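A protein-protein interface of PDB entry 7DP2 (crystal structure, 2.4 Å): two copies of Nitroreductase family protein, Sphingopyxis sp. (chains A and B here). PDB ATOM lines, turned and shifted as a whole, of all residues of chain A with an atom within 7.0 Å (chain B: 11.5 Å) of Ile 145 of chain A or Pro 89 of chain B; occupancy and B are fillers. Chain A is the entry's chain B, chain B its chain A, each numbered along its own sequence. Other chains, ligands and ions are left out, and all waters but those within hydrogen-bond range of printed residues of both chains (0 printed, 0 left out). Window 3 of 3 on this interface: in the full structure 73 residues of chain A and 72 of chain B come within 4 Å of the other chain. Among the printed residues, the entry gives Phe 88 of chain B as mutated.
O of Ile 87 of chain B lies within hydrogen-bond range of NE2 of Gln 150 of chain A (3.0 Å).
NH2 of Arg 99 of chain B lies within hydrogen-bond range of O of Leu 50 of chain A (2.9 Å).
The guanidinium group of Arg 90 of chain B lies within salt-bridge range of the side-chain carboxylate of Asp 86 of chain B, at 2.8 Å.
NE1 of Trp 151 of chain A sits at hydrogen-bond distance from SG of Cys 142 of chain A (3.7 Å).
The backbone NH (N) of Ile 145 of chain A sits close to the side-chain hydroxyl (OG) of Ser 143 of chain A, at 3.4 Å.
OG of Ser 143 of chain A lies close to O of Asp 194 of chain A.
N of Gly 147 of chain A sits at hydrogen-bond distance from OE1 of Gln 150 of chain A.
Among the printed residues, pairs that only touch across the chains: Leu 50 of chain A with Phe 88 of chain B (3.97 Å), Leu 50 of chain A with Leu 92 of chain B (3.8 Å), Leu 50 of chain A with Trp 96 of chain B (3.4 Å), Ser 143 of chain A with Trp 96 of chain B (3.9 Å), Ile 145 of chain A with Pro 89 of chain B (3.5 Å), Ile 145 of chain A with Leu 92 of chain B (3.9 Å), Met 146 of chain A with Trp 96 of chain B (3.3 Å), Pro 148 of chain A with Trp 151 of chain B (3.6 Å), Pro 149 of chain A with Tyr 85 of chain B (3.7 Å), Pro 149 of chain A with Asp 86 of chain B (3.6 Å), Pro 149 of chain A with Ile 87 of chain B (3.3 Å), Pro 149 of chain A with Trp 151 of chain B (3.8 Å), Pro 149 of chain A with Glu 176 of chain B (3.4 Å), Gln 150 of chain A with Phe 88 of chain B (3.99 Å), Gln 150 of chain A with Pro 89 of chain B (3.8 Å) and Trp 151 of chain A with Pro 148 of chain B (3.6 Å).
Ser 143 of chain A touches one residue of chain B.
Met 146 of chain A touches just one residue of chain B: Trp 96 (3.3 Å).
No residue of chain B comes within 4 Å of Gly 147 of chain A.
Of the printed residues of chain B, Trp 151 of chain A touches Pro 148.
Printed residues of chain A within 4 Å of Tyr 85 of chain B: Pro 149.
Printed residues of chain A within 4 Å of Asp 86 of chain B: Pro 149 (3.6 Å).
Of chain A, only Ile 145 (3.5 Å) and Gln 150 (3.8 Å) come within 4 Å of Pro 89 of chain B.
Pro 95 of chain B touches none of the printed residues of chain A.
Of the 22 printed residues of chain B, 11 touch a printed residue of chain A.
Hydrophobic or aromatic side chains of chain B that line the printed part of chain A: Tyr 85, Phe 88, Pro 89, Leu 92, Trp 96, Pro 148 and Trp 151.
Along chain B the printed residues that touch a printed residue of chain A span positions 85 to 176.
Of the 13 printed residues of chain A, 8 touch a printed residue of chain B.
Hydrophobic or aromatic side chains of chain A within 4 Å of the printed part of chain B: Leu 50, Ile 145, Met 146, Pro 148, Pro 149 and Trp 151.
Among the printed residues, no Asp or Glu carboxylate lies within 4 Å of a Lys or Arg side-chain nitrogen of the other chain.
Pro 148 of chain A touches Trp 151 of chain B, and with the chains exchanged Trp 151 of chain A touches Pro 148 of chain B.
Positions printed for both chains: 148 and 151.
Of the 18 pairs that touch across the chains among the printed residues, 2 have their exchanged pair printed and touching as well.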
ATOM      1  N   LEU A  50      24.259   5.976  -1.197  1.00  0.00           N
ATOM      2  CA  LEU A  50      23.533   5.928  -2.438  1.00  0.00           C
ATOM      3  C   LEU A  50      23.241   7.353  -2.906  1.00  0.00           C
ATOM      4  O   LEU A  50      23.144   7.606  -4.106  1.00  0.00           O
ATOM      5  CB  LEU A  50      22.237   5.139  -2.256  1.00  0.00           C
ATOM      6  CG  LEU A  50      22.323   3.608  -2.146  1.00  0.00           C
ATOM      7  CD1 LEU A  50      20.969   3.001  -2.395  1.00  0.00           C
ATOM      8  CD2 LEU A  50      23.333   2.995  -3.111  1.00  0.00           C
ATOM      9  N   CYS A 142      12.936  10.852  -6.684  1.00  0.00           N
ATOM     10  CA  CYS A 142      13.874   9.732  -6.763  1.00  0.00           C
ATOM     11  C   CYS A 142      13.318   8.652  -7.678  1.00  0.00           C
ATOM     12  O   CYS A 142      12.195   8.758  -8.148  1.00  0.00           O
ATOM     13  CB  CYS A 142      14.144   9.144  -5.368  1.00  0.00           C
ATOM     14  SG  CYS A 142      12.708   8.374  -4.499  1.00  0.00           S
ATOM     15  N   SER A 143      14.102   7.615  -7.936  1.00  0.00           N
ATOM     16  CA  SER A 143      13.620   6.529  -8.772  1.00  0.00           C
ATOM     17  C   SER A 143      12.589   5.708  -8.022  1.00  0.00           C
ATOM     18  O   SER A 143      12.681   5.549  -6.807  1.00  0.00           O
ATOM     19  CB  SER A 143      14.759   5.623  -9.244  1.00  0.00           C
ATOM     20  OG  SER A 143      14.217   4.508  -9.929  1.00  0.00           O
ATOM     21  N   ARG A 144      11.636   5.152  -8.765  1.00  0.00           N
ATOM     22  CA  ARG A 144      10.545   4.367  -8.189  1.00  0.00           C
ATOM     23  C   ARG A 144      11.057   3.070  -7.540  1.00  0.00           C
ATOM     24  O   ARG A 144      10.322   2.410  -6.815  1.00  0.00           O
ATOM     25  CB  ARG A 144       9.502   4.063  -9.286  1.00  0.00           C
ATOM     26  CG  ARG A 144       8.128   3.600  -8.806  1.00  0.00           C
ATOM     27  CD  ARG A 144       7.049   3.815  -9.877  1.00  0.00           C
ATOM     28  NE  ARG A 144       6.966   5.215 -10.296  1.00  0.00           N
ATOM     29  CZ  ARG A 144       6.069   6.097  -9.845  1.00  0.00           C
ATOM     30  NH1 ARG A 144       6.098   7.357 -10.276  1.00  0.00           N
ATOM     31  NH2 ARG A 144       5.143   5.732  -8.959  1.00  0.00           N
ATOM     32  N   ILE A 145      12.333   2.751  -7.749  1.00  0.00           N
ATOM     33  CA  ILE A 145      12.948   1.558  -7.168  1.00  0.00           C
ATOM     34  C   ILE A 145      13.342   1.726  -5.697  1.00  0.00           C
ATOM     35  O   ILE A 145      13.377   0.742  -4.939  1.00  0.00           O
ATOM     36  CB  ILE A 145      14.210   1.143  -7.960  1.00  0.00           C
ATOM     37  CG1 ILE A 145      15.280   2.224  -7.824  1.00  0.00           C
ATOM     38  CG2 ILE A 145      13.892   0.965  -9.432  1.00  0.00           C
ATOM     39  CD1 ILE A 145      16.679   1.741  -8.075  1.00  0.00           C
ATOM     40  N   MET A 146      13.611   2.970  -5.300  1.00  0.00           N
ATOM     41  CA  MET A 146      14.052   3.295  -3.945  1.00  0.00           C
ATOM     42  C   MET A 146      13.035   2.856  -2.897  1.00  0.00           C
ATOM     43  O   MET A 146      11.826   2.987  -3.087  1.00  0.00           O
ATOM     44  CB  MET A 146      14.321   4.803  -3.826  1.00  0.00           C
ATOM     45  CG  MET A 146      15.397   5.306  -4.787  1.00  0.00           C
ATOM     46  SD  MET A 146      16.897   4.341  -4.575  1.00  0.00           S
ATOM     47  CE  MET A 146      17.830   4.774  -6.043  1.00  0.00           C
ATOM     48  N   GLY A 147      13.529   2.295  -1.802  1.00  0.00           N
ATOM     49  CA  GLY A 147      12.649   1.846  -0.752  1.00  0.00           C
ATOM     50  C   GLY A 147      12.652   2.859   0.371  1.00  0.00           C
ATOM     51  O   GLY A 147      13.452   3.803   0.357  1.00  0.00           O
ATOM     52  N   PRO A 148      11.804   2.626   1.382  1.00  0.00           N
ATOM     53  CA  PRO A 148      11.625   3.502   2.551  1.00  0.00           C
ATOM     54  C   PRO A 148      12.933   3.931   3.219  1.00  0.00           C
ATOM     55  O   PRO A 148      12.983   5.098   3.585  1.00  0.00           O
ATOM     56  CB  PRO A 148      10.764   2.647   3.508  1.00  0.00           C
ATOM     57  CG  PRO A 148      10.004   1.766   2.600  1.00  0.00           C
ATOM     58  CD  PRO A 148      10.927   1.444   1.445  1.00  0.00           C
ATOM     59  N   PRO A 149      13.948   3.035   3.370  1.00  0.00           N
ATOM     60  CA  PRO A 149      15.223   3.552   3.902  1.00  0.00           C
ATOM     61  C   PRO A 149      15.808   4.697   3.061  1.00  0.00           C
ATOM     62  O   PRO A 149      16.316   5.674   3.628  1.00  0.00           O
ATOM     63  CB  PRO A 149      16.155   2.320   3.857  1.00  0.00           C
ATOM     64  CG  PRO A 149      15.534   1.403   2.877  1.00  0.00           C
ATOM     65  CD  PRO A 149      14.055   1.587   3.058  1.00  0.00           C
ATOM     66  N   GLN A 150      15.717   4.587   1.739  1.00  0.00           N
ATOM     67  CA  GLN A 150      16.204   5.644   0.860  1.00  0.00           C
ATOM     68  C   GLN A 150      15.385   6.930   1.002  1.00  0.00           C
ATOM     69  O   GLN A 150      15.886   8.028   0.762  1.00  0.00           O
ATOM     70  CB  GLN A 150      16.181   5.190  -0.596  1.00  0.00           C
ATOM     71  CG  GLN A 150      17.275   4.188  -0.939  1.00  0.00           C
ATOM     72  CD  GLN A 150      16.963   2.817  -0.399  1.00  0.00           C
ATOM     73  OE1 GLN A 150      15.866   2.304  -0.590  1.00  0.00           O
ATOM     74  NE2 GLN A 150      17.915   2.226   0.300  1.00  0.00           N
ATOM     75  N   TRP A 151      14.126   6.785   1.406  1.00  0.00           N
ATOM     76  CA  TRP A 151      13.276   7.940   1.617  1.00  0.00           C
ATOM     77  C   TRP A 151      13.735   8.640   2.877  1.00  0.00           C
ATOM     78  O   TRP A 151      13.693   9.863   2.973  1.00  0.00           O
ATOM     79  CB  TRP A 151      11.805   7.527   1.694  1.00  0.00           C
ATOM     80  CG  TRP A 151      11.217   7.370   0.352  1.00  0.00           C
ATOM     81  CD1 TRP A 151      11.702   6.609  -0.677  1.00  0.00           C
ATOM     82  CD2 TRP A 151      10.034   8.004  -0.140  1.00  0.00           C
ATOM     83  NE1 TRP A 151      10.887   6.727  -1.779  1.00  0.00           N
ATOM     84  CE2 TRP A 151       9.857   7.581  -1.475  1.00  0.00           C
ATOM     85  CE3 TRP A 151       9.104   8.879   0.421  1.00  0.00           C
ATOM     86  CZ2 TRP A 151       8.784   8.011  -2.259  1.00  0.00           C
ATOM     87  CZ3 TRP A 151       8.044   9.310  -0.356  1.00  0.00           C
ATOM     88  CH2 TRP A 151       7.889   8.876  -1.683  1.00  0.00           C
ATOM     89  N   ASP A 194       9.929   6.750 -14.487  1.00  0.00           N
ATOM     90  CA  ASP A 194      11.007   6.091 -13.767  1.00  0.00           C
ATOM     91  C   ASP A 194      11.193   6.762 -12.402  1.00  0.00           C
ATOM     92  O   ASP A 194      11.835   6.220 -11.497  1.00  0.00           O
ATOM     93  CB  ASP A 194      12.293   6.147 -14.595  1.00  0.00           C
ATOM     94  CG  ASP A 194      12.782   7.575 -14.838  1.00  0.00           C
ATOM     95  OD1 ASP A 194      12.180   8.312 -15.651  1.00  0.00           O
ATOM     96  OD2 ASP A 194      13.791   7.959 -14.213  1.00  0.00           O
ATOM     97  N   ILE A 196       9.561   9.111  -9.028  1.00  0.00           N
ATOM     98  CA  ILE A 196       8.385   9.408  -8.206  1.00  0.00           C
ATOM     99  C   ILE A 196       8.617  10.700  -7.412  1.00  0.00           C
ATOM    100  O   ILE A 196       9.723  10.943  -6.918  1.00  0.00           O
ATOM    101  CB  ILE A 196       8.016   8.257  -7.231  1.00  0.00           C
ATOM    102  CG1 ILE A 196       6.912   8.726  -6.268  1.00  0.00           C
ATOM    103  CG2 ILE A 196       9.215   7.846  -6.406  1.00  0.00           C
ATOM    104  CD1 ILE A 196       6.259   7.651  -5.423  1.00  0.00           C
ATOM    105  N   PRO B  83      15.413  -9.804   8.343  1.00  0.00           N
ATOM    106  CA  PRO B  83      15.333  -8.473   7.747  1.00  0.00           C
ATOM    107  C   PRO B  83      13.996  -7.782   8.050  1.00  0.00           C
ATOM    108  O   PRO B  83      12.963  -8.366   7.727  1.00  0.00           O
ATOM    109  CB  PRO B  83      15.466  -8.760   6.245  1.00  0.00           C
ATOM    110  CG  PRO B  83      15.975 -10.160   6.152  1.00  0.00           C
ATOM    111  CD  PRO B  83      15.408 -10.863   7.323  1.00  0.00           C
ATOM    112  N   TYR B  85      13.059  -5.177   6.484  1.00  0.00           N
ATOM    113  CA  TYR B  85      12.704  -4.631   5.174  1.00  0.00           C
ATOM    114  C   TYR B  85      13.938  -4.792   4.290  1.00  0.00           C
ATOM    115  O   TYR B  85      14.985  -5.252   4.764  1.00  0.00           O
ATOM    116  CB  TYR B  85      12.304  -3.141   5.264  1.00  0.00           C
ATOM    117  CG  TYR B  85      13.395  -2.282   5.887  1.00  0.00           C
ATOM    118  CD1 TYR B  85      14.409  -1.730   5.107  1.00  0.00           C
ATOM    119  CD2 TYR B  85      13.433  -2.051   7.259  1.00  0.00           C
ATOM    120  CE1 TYR B  85      15.422  -0.966   5.683  1.00  0.00           C
ATOM    121  CE2 TYR B  85      14.447  -1.287   7.849  1.00  0.00           C
ATOM    122  CZ  TYR B  85      15.434  -0.746   7.059  1.00  0.00           C
ATOM    123  OH  TYR B  85      16.443   0.008   7.640  1.00  0.00           O
ATOM    124  N   ASP B  86      13.843  -4.367   3.033  1.00  0.00           N
ATOM    125  CA  ASP B  86      14.991  -4.430   2.138  1.00  0.00           C
ATOM    126  C   ASP B  86      15.842  -3.188   2.283  1.00  0.00           C
ATOM    127  O   ASP B  86      15.427  -2.072   1.926  1.00  0.00           O
ATOM    128  CB  ASP B  86      14.560  -4.582   0.686  1.00  0.00           C
ATOM    129  CG  ASP B  86      14.047  -5.958   0.374  1.00  0.00           C
ATOM    130  OD1 ASP B  86      14.853  -6.913   0.361  1.00  0.00           O
ATOM    131  OD2 ASP B  86      12.829  -6.088   0.160  1.00  0.00           O
ATOM    132  N   ILE B  87      17.024  -3.392   2.852  1.00  0.00           N
ATOM    133  CA  ILE B  87      17.938  -2.301   3.129  1.00  0.00           C
ATOM    134  C   ILE B  87      18.242  -1.610   1.808  1.00  0.00           C
ATOM    135  O   ILE B  87      18.045  -0.407   1.642  1.00  0.00           O
ATOM    136  CB  ILE B  87      19.224  -2.801   3.822  1.00  0.00           C
ATOM    137  CG1 ILE B  87      18.895  -3.252   5.252  1.00  0.00           C
ATOM    138  CG2 ILE B  87      20.291  -1.709   3.826  1.00  0.00           C
ATOM    139  CD1 ILE B  87      19.999  -4.030   5.970  1.00  0.00           C
ATOM    140  N   PHE B  88      18.730  -2.387   0.859  1.00  0.00           N
ATOM    141  CA  PHE B  88      18.922  -1.877  -0.476  1.00  0.00           C
ATOM    142  C   PHE B  88      17.888  -2.488  -1.393  1.00  0.00           C
ATOM    143  O   PHE B  88      17.395  -3.585  -1.132  1.00  0.00           O
ATOM    144  CB  PHE B  88      20.347  -2.153  -0.944  1.00  0.00           C
ATOM    145  CG  PHE B  88      21.370  -1.405  -0.150  1.00  0.00           C
ATOM    146  CD1 PHE B  88      21.187  -0.057   0.125  1.00  0.00           C
ATOM    147  CD2 PHE B  88      22.460  -2.053   0.391  1.00  0.00           C
ATOM    148  CE1 PHE B  88      22.099   0.650   0.888  1.00  0.00           C
ATOM    149  CE2 PHE B  88      23.380  -1.355   1.164  1.00  0.00           C
ATOM    150  CZ  PHE B  88      23.198   0.000   1.413  1.00  0.00           C
ATOM    151  N   PRO B  89      17.506  -1.750  -2.440  1.00  0.00           N
ATOM    152  CA  PRO B  89      16.567  -2.298  -3.431  1.00  0.00           C
ATOM    153  C   PRO B  89      17.185  -3.490  -4.175  1.00  0.00           C
ATOM    154  O   PRO B  89      18.244  -3.353  -4.785  1.00  0.00           O
ATOM    155  CB  PRO B  89      16.312  -1.119  -4.381  1.00  0.00           C
ATOM    156  CG  PRO B  89      16.713   0.117  -3.552  1.00  0.00           C
ATOM    157  CD  PRO B  89      17.839  -0.338  -2.686  1.00  0.00           C
ATOM    158  N   ARG B  90      16.558  -4.657  -4.051  1.00  0.00           N
ATOM    159  CA  ARG B  90      16.900  -5.824  -4.858  1.00  0.00           C
ATOM    160  C   ARG B  90      17.065  -5.467  -6.319  1.00  0.00           C
ATOM    161  O   ARG B  90      16.188  -4.832  -6.907  1.00  0.00           O
ATOM    162  CB  ARG B  90      15.844  -6.909  -4.706  1.00  0.00           C
ATOM    163  CG  ARG B  90      15.549  -7.296  -3.276  1.00  0.00           C
ATOM    164  CD  ARG B  90      14.259  -8.099  -3.200  1.00  0.00           C
ATOM    165  NE  ARG B  90      13.840  -8.311  -1.817  1.00  0.00           N
ATOM    166  CZ  ARG B  90      13.958  -9.478  -1.187  1.00  0.00           C
ATOM    167  NH1 ARG B  90      13.574  -9.600   0.080  1.00  0.00           N
ATOM    168  NH2 ARG B  90      14.455 -10.533  -1.831  1.00  0.00           N
ATOM    169  N   GLY B  91      18.209  -5.838  -6.889  1.00  0.00           N
ATOM    170  CA  GLY B  91      18.486  -5.512  -8.271  1.00  0.00           C
ATOM    171  C   GLY B  91      18.749  -4.023  -8.374  1.00  0.00           C
ATOM    172  O   GLY B  91      18.325  -3.386  -9.336  1.00  0.00           O
ATOM    173  N   LEU B  92      19.432  -3.463  -7.375  1.00  0.00           N
ATOM    174  CA  LEU B  92      19.842  -2.063  -7.428  1.00  0.00           C
ATOM    175  C   LEU B  92      20.691  -1.864  -8.672  1.00  0.00           C
ATOM    176  O   LEU B  92      21.656  -2.597  -8.902  1.00  0.00           O
ATOM    177  CB  LEU B  92      20.617  -1.685  -6.164  1.00  0.00           C
ATOM    178  CG  LEU B  92      21.012  -0.240  -5.858  1.00  0.00           C
ATOM    179  CD1 LEU B  92      19.800   0.677  -5.992  1.00  0.00           C
ATOM    180  CD2 LEU B  92      21.602  -0.141  -4.449  1.00  0.00           C
ATOM    181  N   THR B  93      20.320  -0.886  -9.490  1.00  0.00           N
ATOM    182  CA  THR B  93      21.005  -0.702 -10.765  1.00  0.00           C
ATOM    183  C   THR B  93      22.311   0.050 -10.617  1.00  0.00           C
ATOM    184  O   THR B  93      22.581   0.700  -9.604  1.00  0.00           O
ATOM    185  CB  THR B  93      20.125  -0.006 -11.830  1.00  0.00           C
ATOM    186  OG1 THR B  93      19.776   1.312 -11.404  1.00  0.00           O
ATOM    187  CG2 THR B  93      18.865  -0.812 -12.086  1.00  0.00           C
ATOM    188  N   ASP B  94      23.096  -0.058 -11.678  1.00  0.00           N
ATOM    189  CA  ASP B  94      24.488   0.359 -11.741  1.00  0.00           C
ATOM    190  C   ASP B  94      24.845   1.820 -11.448  1.00  0.00           C
ATOM    191  O   ASP B  94      26.006   2.083 -11.129  1.00  0.00           O
ATOM    192  CB  ASP B  94      25.008  -0.005 -13.135  1.00  0.00           C
ATOM    193  CG  ASP B  94      25.022  -1.505 -13.359  1.00  0.00           C
ATOM    194  OD1 ASP B  94      24.503  -2.204 -12.453  1.00  0.00           O
ATOM    195  OD2 ASP B  94      25.502  -1.983 -14.425  1.00  0.00           O
ATOM    196  N   PRO B  95      23.899   2.776 -11.597  1.00  0.00           N
ATOM    197  CA  PRO B  95      24.234   4.110 -11.078  1.00  0.00           C
ATOM    198  C   PRO B  95      24.617   4.124  -9.605  1.00  0.00           C
ATOM    199  O   PRO B  95      25.746   4.435  -9.220  1.00  0.00           O
ATOM    200  CB  PRO B  95      22.925   4.882 -11.267  1.00  0.00           C
ATOM    201  CG  PRO B  95      22.365   4.309 -12.509  1.00  0.00           C
ATOM    202  CD  PRO B  95      22.687   2.828 -12.439  1.00  0.00           C
ATOM    203  N   TRP B  96      23.645   3.720  -8.798  1.00  0.00           N
ATOM    204  CA  TRP B  96      23.745   3.761  -7.354  1.00  0.00           C
ATOM    205  C   TRP B  96      24.642   2.656  -6.845  1.00  0.00           C
ATOM    206  O   TRP B  96      25.352   2.816  -5.854  1.00  0.00           O
ATOM    207  CB  TRP B  96      22.346   3.660  -6.738  1.00  0.00           C
ATOM    208  CG  TRP B  96      21.432   4.785  -7.159  1.00  0.00           C
ATOM    209  CD1 TRP B  96      21.327   6.008  -6.579  1.00  0.00           C
ATOM    210  CD2 TRP B  96      20.503   4.767  -8.254  1.00  0.00           C
ATOM    211  NE1 TRP B  96      20.396   6.766  -7.245  1.00  0.00           N
ATOM    212  CE2 TRP B  96      19.875   6.038  -8.270  1.00  0.00           C
ATOM    213  CE3 TRP B  96      20.146   3.821  -9.226  1.00  0.00           C
ATOM    214  CZ2 TRP B  96      18.894   6.367  -9.213  1.00  0.00           C
ATOM    215  CZ3 TRP B  96      19.174   4.152 -10.169  1.00  0.00           C
ATOM    216  CH2 TRP B  96      18.560   5.423 -10.152  1.00  0.00           C
ATOM    217  N   ASP B  97      24.598   1.525  -7.535  1.00  0.00           N
ATOM    218  CA  ASP B  97      25.368   0.363  -7.139  1.00  0.00           C
ATOM    219  C   ASP B  97      26.870   0.710  -7.028  1.00  0.00           C
ATOM    220  O   ASP B  97      27.565   0.189  -6.155  1.00  0.00           O
ATOM    221  CB  ASP B  97      25.137  -0.760  -8.155  1.00  0.00           C
ATOM    222  CG  ASP B  97      25.796  -2.052  -7.759  1.00  0.00           C
ATOM    223  OD1 ASP B  97      25.897  -2.274  -6.534  1.00  0.00           O
ATOM    224  OD2 ASP B  97      26.180  -2.844  -8.659  1.00  0.00           O
ATOM    225  N   SER B  98      27.359   1.595  -7.899  1.00  0.00           N
ATOM    226  CA  SER B  98      28.752   2.069  -7.856  1.00  0.00           C
ATOM    227  C   SER B  98      29.091   2.934  -6.630  1.00  0.00           C
ATOM    228  O   SER B  98      30.168   2.825  -6.044  1.00  0.00           O
ATOM    229  CB  SER B  98      29.070   2.846  -9.132  1.00  0.00           C
ATOM    230  OG  SER B  98      28.483   2.223 -10.268  1.00  0.00           O
ATOM    231  N   ARG B  99      28.156   3.790  -6.236  1.00  0.00           N
ATOM    232  CA  ARG B  99      28.375   4.665  -5.097  1.00  0.00           C
ATOM    233  C   ARG B  99      28.602   3.837  -3.833  1.00  0.00           C
ATOM    234  O   ARG B  99      29.493   4.144  -3.032  1.00  0.00           O
ATOM    235  CB  ARG B  99      27.188   5.617  -4.931  1.00  0.00           C
ATOM    236  CG  ARG B  99      26.855   6.382  -6.215  1.00  0.00           C
ATOM    237  CD  ARG B  99      25.578   7.219  -6.088  1.00  0.00           C
ATOM    238  NE  ARG B  99      25.304   7.951  -7.325  1.00  0.00           N
ATOM    239  CZ  ARG B  99      24.320   8.835  -7.498  1.00  0.00           C
ATOM    240  NH1 ARG B  99      24.169   9.428  -8.680  1.00  0.00           N
ATOM    241  NH2 ARG B  99      23.486   9.120  -6.501  1.00  0.00           N
ATOM    242  N   ARG B 100      27.822   2.766  -3.684  1.00  0.00           N
ATOM    243  CA  ARG B 100      27.915   1.896  -2.512  1.00  0.00           C
ATOM    244  C   ARG B 100      29.287   1.251  -2.335  1.00  0.00           C
ATOM    245  O   ARG B 100      29.865   1.289  -1.251  1.00  0.00           O
ATOM    246  CB  ARG B 100      26.822   0.821  -2.562  1.00  0.00           C
ATOM    247  CG  ARG B 100      26.817  -0.085  -1.350  1.00  0.00           C
ATOM    248  CD  ARG B 100      25.632  -1.037  -1.331  1.00  0.00           C
ATOM    249  NE  ARG B 100      25.410  -1.799  -2.554  1.00  0.00           N
ATOM    250  CZ  ARG B 100      24.835  -2.996  -2.581  1.00  0.00           C
ATOM    251  NH1 ARG B 100      24.639  -3.625  -3.735  1.00  0.00           N
ATOM    252  NH2 ARG B 100      24.464  -3.570  -1.442  1.00  0.00           N
ATOM    253  N   PHE B 101      29.796   0.638  -3.388  1.00  0.00           N
ATOM    254  CA  PHE B 101      31.088  -0.017  -3.307  1.00  0.00           C
ATOM    255  C   PHE B 101      32.215   1.000  -3.404  1.00  0.00           C
ATOM    256  O   PHE B 101      33.311   0.768  -2.901  1.00  0.00           O
ATOM    257  CB  PHE B 101      31.180  -1.120  -4.368  1.00  0.00           C
ATOM    258  CG  PHE B 101      30.150  -2.194  -4.165  1.00  0.00           C
ATOM    259  CD1 PHE B 101      30.284  -3.106  -3.125  1.00  0.00           C
ATOM    260  CD2 PHE B 101      29.009  -2.247  -4.952  1.00  0.00           C
ATOM    261  CE1 PHE B 101      29.319  -4.083  -2.901  1.00  0.00           C
ATOM    262  CE2 PHE B 101      28.042  -3.222  -4.733  1.00  0.00           C
ATOM    263  CZ  PHE B 101      28.199  -4.143  -3.706  1.00  0.00           C
ATOM    264  N   PRO B 148       6.269   5.672   3.821  1.00  0.00           N
ATOM    265  CA  PRO B 148       7.553   6.251   3.386  1.00  0.00           C
ATOM    266  C   PRO B 148       7.743   7.775   3.686  1.00  0.00           C
ATOM    267  O   PRO B 148       8.820   8.170   4.126  1.00  0.00           O
ATOM    268  CB  PRO B 148       7.554   5.974   1.868  1.00  0.00           C
ATOM    269  CG  PRO B 148       6.657   4.797   1.692  1.00  0.00           C
ATOM    270  CD  PRO B 148       5.572   4.946   2.738  1.00  0.00           C
ATOM    271  N   TRP B 151       8.927   7.988   6.906  1.00  0.00           N
ATOM    272  CA  TRP B 151      10.301   7.519   7.015  1.00  0.00           C
ATOM    273  C   TRP B 151      11.205   8.667   6.644  1.00  0.00           C
ATOM    274  O   TRP B 151      12.265   8.851   7.248  1.00  0.00           O
ATOM    275  CB  TRP B 151      10.551   6.293   6.136  1.00  0.00           C
ATOM    276  CG  TRP B 151      10.073   5.054   6.803  1.00  0.00           C
ATOM    277  CD1 TRP B 151       8.826   4.832   7.333  1.00  0.00           C
ATOM    278  CD2 TRP B 151      10.820   3.853   7.025  1.00  0.00           C
ATOM    279  NE1 TRP B 151       8.762   3.574   7.875  1.00  0.00           N
ATOM    280  CE2 TRP B 151       9.971   2.952   7.698  1.00  0.00           C
ATOM    281  CE3 TRP B 151      12.123   3.457   6.721  1.00  0.00           C
ATOM    282  CZ2 TRP B 151      10.384   1.680   8.074  1.00  0.00           C
ATOM    283  CZ3 TRP B 151      12.527   2.197   7.086  1.00  0.00           C
ATOM    284  CH2 TRP B 151      11.656   1.315   7.747  1.00  0.00           C
ATOM    285  N   GLU B 176      22.139   0.659   9.430  1.00  0.00           N
ATOM    286  CA  GLU B 176      20.994  -0.122   8.986  1.00  0.00           C
ATOM    287  C   GLU B 176      21.233  -1.606   9.242  1.00  0.00           C
ATOM    288  O   GLU B 176      20.325  -2.420   9.100  1.00  0.00           O
ATOM    289  CB  GLU B 176      20.734   0.088   7.502  1.00  0.00           C
ATOM    290  CG  GLU B 176      19.764   1.191   7.186  1.00  0.00           C
ATOM    291  CD  GLU B 176      19.979   1.792   5.797  1.00  0.00           C
ATOM    292  OE1 GLU B 176      20.966   1.446   5.114  1.00  0.00           O
ATOM    293  OE2 GLU B 176      19.157   2.628   5.393  1.00  0.00           O
ATOM    294  N   MET B 180      18.944  -6.095   9.787  1.00  0.00           N
ATOM    295  CA  MET B 180      19.178  -7.497   9.420  1.00  0.00           C
ATOM    296  C   MET B 180      18.675  -8.462  10.486  1.00  0.00           C
ATOM    297  O   MET B 180      18.545  -9.658  10.219  1.00  0.00           O
ATOM    298  CB  MET B 180      20.667  -7.775   9.183  1.00  0.00           C
ATOM    299  CG  MET B 180      21.264  -7.024   8.022  1.00  0.00           C
ATOM    300  SD  MET B 180      20.392  -7.460   6.532  1.00  0.00           S
ATOM    301  CE  MET B 180      20.648  -9.228   6.509  1.00  0.00           C
